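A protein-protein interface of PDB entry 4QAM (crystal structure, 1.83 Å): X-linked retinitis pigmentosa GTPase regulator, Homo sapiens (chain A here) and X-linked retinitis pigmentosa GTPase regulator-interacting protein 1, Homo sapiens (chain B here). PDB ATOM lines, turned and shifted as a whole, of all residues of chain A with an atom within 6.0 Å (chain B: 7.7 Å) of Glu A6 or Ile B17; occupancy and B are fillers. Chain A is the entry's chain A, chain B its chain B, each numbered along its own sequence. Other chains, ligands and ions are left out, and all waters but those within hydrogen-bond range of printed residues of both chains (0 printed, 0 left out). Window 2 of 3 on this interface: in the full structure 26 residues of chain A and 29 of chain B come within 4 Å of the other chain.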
ATOM      1  N   GLU A   6     -21.684  13.657  17.331  1.00  0.00           N
ATOM      2  CA  GLU A   6     -22.777  14.370  18.089  1.00  0.00           C
ATOM      3  C   GLU A   6     -23.940  15.034  17.267  1.00  0.00           C
ATOM      4  O   GLU A   6     -25.007  14.409  17.105  1.00  0.00           O
ATOM      5  CB  GLU A   6     -22.166  15.326  19.114  1.00  0.00           C
ATOM      6  CG  GLU A   6     -21.857  14.615  20.415  1.00  0.00           C
ATOM      7  CD  GLU A   6     -22.211  15.444  21.638  1.00  0.00           C
ATOM      8  OE1 GLU A   6     -23.317  16.033  21.698  1.00  0.00           O
ATOM      9  OE2 GLU A   6     -21.373  15.491  22.558  1.00  0.00           O
ATOM     10  N   LEU A   7     -23.783  16.272  16.775  1.00  0.00           N
ATOM     11  CA  LEU A   7     -24.802  16.861  15.856  1.00  0.00           C
ATOM     12  C   LEU A   7     -24.622  16.174  14.491  1.00  0.00           C
ATOM     13  O   LEU A   7     -23.468  15.965  14.096  1.00  0.00           O
ATOM     14  CB  LEU A   7     -24.603  18.383  15.704  1.00  0.00           C
ATOM     15  CG  LEU A   7     -25.652  19.404  15.172  1.00  0.00           C
ATOM     16  CD1 LEU A   7     -25.607  20.669  16.022  1.00  0.00           C
ATOM     17  CD2 LEU A   7     -25.549  19.805  13.695  1.00  0.00           C
ATOM     18  N   MET A   8     -25.716  15.802  13.790  1.00  0.00           N
ATOM     19  CA  MET A   8     -25.590  15.299  12.397  1.00  0.00           C
ATOM     20  C   MET A   8     -24.893  16.340  11.527  1.00  0.00           C
ATOM     21  O   MET A   8     -25.341  17.483  11.442  1.00  0.00           O
ATOM     22  CB  MET A   8     -26.915  14.921  11.753  1.00  0.00           C
ATOM     23  CG  MET A   8     -26.723  14.278  10.382  1.00  0.00           C
ATOM     24  SD  MET A   8     -28.101  14.369   9.251  1.00  0.00           S
ATOM     25  CE  MET A   8     -29.373  13.587  10.236  1.00  0.00           C
ATOM     26  N   LYS A  29     -29.273   5.363  11.724  1.00  0.00           N
ATOM     27  CA  LYS A  29     -28.610   6.464  11.129  1.00  0.00           C
ATOM     28  C   LYS A  29     -27.164   6.390  11.668  1.00  0.00           C
ATOM     29  O   LYS A  29     -26.940   6.019  12.866  1.00  0.00           O
ATOM     30  CB  LYS A  29     -29.378   7.729  11.643  1.00  0.00           C
ATOM     31  CG  LYS A  29     -28.840   9.085  11.249  1.00  0.00           C
ATOM     32  CD  LYS A  29     -29.727  10.290  11.644  1.00  0.00           C
ATOM     33  CE  LYS A  29     -30.348  10.249  13.049  1.00  0.00           C
ATOM     34  NZ  LYS A  29     -30.586  11.617  13.664  1.00  0.00           N
ATOM     35  N   PHE A  30     -26.196   6.701  10.802  1.00  0.00           N
ATOM     36  CA  PHE A  30     -24.806   6.812  11.207  1.00  0.00           C
ATOM     37  C   PHE A  30     -24.044   7.713  10.236  1.00  0.00           C
ATOM     38  O   PHE A  30     -24.545   8.000   9.120  1.00  0.00           O
ATOM     39  CB  PHE A  30     -24.210   5.437  11.328  1.00  0.00           C
ATOM     40  CG  PHE A  30     -23.983   4.722  10.035  1.00  0.00           C
ATOM     41  CD1 PHE A  30     -24.956   3.831   9.522  1.00  0.00           C
ATOM     42  CD2 PHE A  30     -22.801   4.906   9.339  1.00  0.00           C
ATOM     43  CE1 PHE A  30     -24.700   3.127   8.352  1.00  0.00           C
ATOM     44  CE2 PHE A  30     -22.550   4.234   8.158  1.00  0.00           C
ATOM     45  CZ  PHE A  30     -23.503   3.342   7.659  1.00  0.00           C
ATOM     46  N   TRP A  31     -22.844   8.143  10.642  1.00  0.00           N
ATOM     47  CA  TRP A  31     -21.976   8.840   9.756  1.00  0.00           C
ATOM     48  C   TRP A  31     -20.542   8.613  10.207  1.00  0.00           C
ATOM     49  O   TRP A  31     -20.287   7.794  11.084  1.00  0.00           O
ATOM     50  CB  TRP A  31     -22.336  10.347   9.685  1.00  0.00           C
ATOM     51  CG  TRP A  31     -22.294  11.061  11.033  1.00  0.00           C
ATOM     52  CD1 TRP A  31     -21.190  11.652  11.656  1.00  0.00           C
ATOM     53  CD2 TRP A  31     -23.418  11.273  11.942  1.00  0.00           C
ATOM     54  NE1 TRP A  31     -21.555  12.217  12.859  1.00  0.00           N
ATOM     55  CE2 TRP A  31     -22.876  12.013  13.099  1.00  0.00           C
ATOM     56  CE3 TRP A  31     -24.799  10.915  11.920  1.00  0.00           C
ATOM     57  CZ2 TRP A  31     -23.672  12.391  14.166  1.00  0.00           C
ATOM     58  CZ3 TRP A  31     -25.622  11.336  13.014  1.00  0.00           C
ATOM     59  CH2 TRP A  31     -25.055  12.040  14.113  1.00  0.00           C
ATOM     60  N   PHE A  32     -19.610   9.312   9.583  1.00  0.00           N
ATOM     61  CA  PHE A  32     -18.216   9.041   9.792  1.00  0.00           C
ATOM     62  C   PHE A  32     -17.513  10.250  10.361  1.00  0.00           C
ATOM     63  O   PHE A  32     -17.908  11.391  10.136  1.00  0.00           O
ATOM     64  CB  PHE A  32     -17.563   8.700   8.467  1.00  0.00           C
ATOM     65  CG  PHE A  32     -18.107   7.468   7.822  1.00  0.00           C
ATOM     66  CD1 PHE A  32     -17.657   6.198   8.219  1.00  0.00           C
ATOM     67  CD2 PHE A  32     -19.075   7.560   6.778  1.00  0.00           C
ATOM     68  CE1 PHE A  32     -18.198   5.067   7.629  1.00  0.00           C
ATOM     69  CE2 PHE A  32     -19.573   6.410   6.148  1.00  0.00           C
ATOM     70  CZ  PHE A  32     -19.167   5.167   6.600  1.00  0.00           C
ATOM     71  N   LYS A  33     -16.448  10.025  11.104  1.00  0.00           N
ATOM     72  CA  LYS A  33     -15.690  11.174  11.631  1.00  0.00           C
ATOM     73  C   LYS A  33     -14.834  11.741  10.475  1.00  0.00           C
ATOM     74  O   LYS A  33     -14.068  11.003   9.868  1.00  0.00           O
ATOM     75  CB  LYS A  33     -14.839  10.646  12.766  1.00  0.00           C
ATOM     76  CG  LYS A  33     -14.069  11.736  13.537  1.00  0.00           C
ATOM     77  CD  LYS A  33     -12.769  11.117  14.019  1.00  0.00           C
ATOM     78  CE  LYS A  33     -11.778  12.119  14.613  1.00  0.00           C
ATOM     79  NZ  LYS A  33     -12.376  12.596  15.890  1.00  0.00           N
ATOM     80  N   LYS A  77     -22.731  -3.425  13.405  1.00  0.00           N
ATOM     81  CA  LYS A  77     -22.330  -2.042  13.159  1.00  0.00           C
ATOM     82  C   LYS A  77     -21.542  -2.022  11.827  1.00  0.00           C
ATOM     83  O   LYS A  77     -20.699  -2.914  11.560  1.00  0.00           O
ATOM     84  CB  LYS A  77     -21.341  -1.672  14.309  1.00  0.00           C
ATOM     85  CG  LYS A  77     -21.162  -0.247  14.753  1.00  0.00           C
ATOM     86  CD  LYS A  77     -19.990  -0.276  15.731  1.00  0.00           C
ATOM     87  CE  LYS A  77     -20.037   0.799  16.804  1.00  0.00           C
ATOM     88  NZ  LYS A  77     -19.539   2.117  16.314  1.00  0.00           N
ATOM     89  N   ASP B  14     -11.407   4.795  12.827  1.00  0.00           N
ATOM     90  CA  ASP B  14     -12.099   3.993  11.816  1.00  0.00           C
ATOM     91  C   ASP B  14     -13.505   3.779  12.417  1.00  0.00           C
ATOM     92  O   ASP B  14     -14.154   2.762  12.149  1.00  0.00           O
ATOM     93  CB  ASP B  14     -11.434   2.635  11.606  1.00  0.00           C
ATOM     94  CG  ASP B  14     -10.101   2.725  10.848  1.00  0.00           C
ATOM     95  OD1 ASP B  14      -9.916   3.643  10.014  1.00  0.00           O
ATOM     96  OD2 ASP B  14      -9.237   1.858  11.093  1.00  0.00           O
ATOM     97  N   ASP B  15     -13.946   4.731  13.243  1.00  0.00           N
ATOM     98  CA  ASP B  15     -15.200   4.633  13.972  1.00  0.00           C
ATOM     99  C   ASP B  15     -16.319   5.424  13.309  1.00  0.00           C
ATOM    100  O   ASP B  15     -16.153   6.543  12.809  1.00  0.00           O
ATOM    101  CB  ASP B  15     -15.040   5.024  15.461  1.00  0.00           C
ATOM    102  CG  ASP B  15     -14.560   3.844  16.345  1.00  0.00           C
ATOM    103  OD1 ASP B  15     -14.976   2.671  16.169  1.00  0.00           O
ATOM    104  OD2 ASP B  15     -13.749   4.109  17.246  1.00  0.00           O
ATOM    105  N   VAL B  16     -17.443   4.756  13.238  1.00  0.00           N
ATOM    106  CA  VAL B  16     -18.642   5.329  12.718  1.00  0.00           C
ATOM    107  C   VAL B  16     -19.300   5.932  13.953  1.00  0.00           C
ATOM    108  O   VAL B  16     -19.023   5.489  15.074  1.00  0.00           O
ATOM    109  CB  VAL B  16     -19.407   4.294  11.898  1.00  0.00           C
ATOM    110  CG1 VAL B  16     -18.355   3.339  11.323  1.00  0.00           C
ATOM    111  CG2 VAL B  16     -20.498   3.562  12.660  1.00  0.00           C
ATOM    112  N   ILE B  17     -20.013   7.033  13.763  1.00  0.00           N
ATOM    113  CA  ILE B  17     -20.650   7.739  14.866  1.00  0.00           C
ATOM    114  C   ILE B  17     -22.060   7.302  14.763  1.00  0.00           C
ATOM    115  O   ILE B  17     -22.653   7.330  13.661  1.00  0.00           O
ATOM    116  CB  ILE B  17     -20.478   9.261  14.710  1.00  0.00           C
ATOM    117  CG1 ILE B  17     -18.984   9.580  14.671  1.00  0.00           C
ATOM    118  CG2 ILE B  17     -21.209  10.005  15.821  1.00  0.00           C
ATOM    119  CD1 ILE B  17     -18.596  11.045  14.750  1.00  0.00           C
ATOM    120  N   VAL B  18     -22.584   6.757  15.849  1.00  0.00           N
ATOM    121  CA  VAL B  18     -23.989   6.362  15.848  1.00  0.00           C
ATOM    122  C   VAL B  18     -24.656   7.259  16.881  1.00  0.00           C
ATOM    123  O   VAL B  18     -24.254   7.246  18.057  1.00  0.00           O
ATOM    124  CB  VAL B  18     -24.166   4.870  16.168  1.00  0.00           C
ATOM    125  CG1 VAL B  18     -25.640   4.439  16.061  1.00  0.00           C
ATOM    126  CG2 VAL B  18     -23.274   4.022  15.243  1.00  0.00           C
ATOM    127  N   PRO B  19     -25.600   8.126  16.456  1.00  0.00           N
ATOM    128  CA  PRO B  19     -26.242   8.994  17.469  1.00  0.00           C
ATOM    129  C   PRO B  19     -27.179   8.147  18.391  1.00  0.00           C
ATOM    130  O   PRO B  19     -27.525   7.001  18.026  1.00  0.00           O
ATOM    131  CB  PRO B  19     -27.039   9.969  16.601  1.00  0.00           C
ATOM    132  CG  PRO B  19     -27.465   9.087  15.467  1.00  0.00           C
ATOM    133  CD  PRO B  19     -26.209   8.304  15.138  1.00  0.00           C
ATOM    134  N   PRO B  20     -27.575   8.678  19.576  1.00  0.00           N
ATOM    135  CA  PRO B  20     -28.532   7.938  20.432  1.00  0.00           C
ATOM    136  C   PRO B  20     -29.875   7.827  19.770  1.00  0.00           C
ATOM    137  O   PRO B  20     -30.185   8.622  18.893  1.00  0.00           O
ATOM    138  CB  PRO B  20     -28.659   8.824  21.678  1.00  0.00           C
ATOM    139  CG  PRO B  20     -27.456   9.700  21.676  1.00  0.00           C
ATOM    140  CD  PRO B  20     -27.045   9.885  20.253  1.00  0.00           C
ATOM    141  N   MET B  21     -30.674   6.838  20.131  1.00  0.00           N
ATOM    142  CA  MET B  21     -32.037   6.763  19.559  1.00  0.00           C
ATOM    143  C   MET B  21     -32.882   6.061  20.583  1.00  0.00           C
ATOM    144  O   MET B  21     -34.017   5.685  20.303  1.00  0.00           O
ATOM    145  CB  MET B  21     -32.189   6.096  18.169  1.00  0.00           C
ATOM    146  CG  MET B  21     -31.249   6.515  17.022  1.00  0.00           C
ATOM    147  SD  MET B  21     -30.704   4.926  15.949  1.00  0.00           S
ATOM    148  CE  MET B  21     -28.981   5.408  15.136  1.00  0.00           C
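The backbone NH of Ile B17 is in hydrogen-bond range of the backbone carbonyl oxygen of Trp A31 (2.8 Å).
Among the printed residues, merely in contact across the chains: Lys A29 with Met B21 (3.1 Å), Lys A29 with Pro B19 (3.3 Å), Phe A30 with Ile B17 (3.3 Å), Trp A31 with Val B16 (3.4 Å), Lys A77 with Val B16 (3.6 Å), Trp A31 with Pro B19 (3.7 Å), Lys A29 with Val B18 (3.8 Å), Lys A33 with Asp B15 (3.9 Å) and Glu A6 with Ile B17 (3.98 Å).
Of the printed residues of chain B, Glu A6 touches Ile B17 (3.98 Å). Of the printed residues of chain A, Ile B17 touches Glu A6 (3.98 Å), Phe A30 (3.3 Å) and Trp A31 (2.8 Å). Printed residues of chain A within 4 Å of Val B18: Lys A29 (3.8 Å). Of the printed residues of chain A, Pro B19 touches Lys A29 and Trp A31. Of the printed residues of chain B, Lys A29 touches Val B18, Pro B19 and Met B21. Printed residues of chain A within 4 Å of Met B21: Lys A29. Pro B20 touches none of the printed residues of chain A. Leu A7 touches none of the printed residues of chain B. The nearest printed residue of chain B that does not touch Glu A6 is Pro B19 (4.9 Å). The nearest printed residue of chain A that does not touch Ile B17 is Lys A33 (4.3 Å).
Of the 9 printed residues of chain A, 6 touch a printed residue of chain B. Hydrophobic or aromatic side chains of chain A within 4 Å of the printed part of chain B: Phe A30 and Trp A31. Along chain A the printed residues that touch a printed residue of chain B span positions 6 to 77. Printed residues of chain B that touch a printed residue of chain A: Asp B15, Val B16, Ile B17, Val B18, Pro B19 and Met B21. Hydrophobic or aromatic side chains of chain B within 4 Å of the printed part of chain A: Val B16, Ile B17, Val B18, Pro B19 and Met B21.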
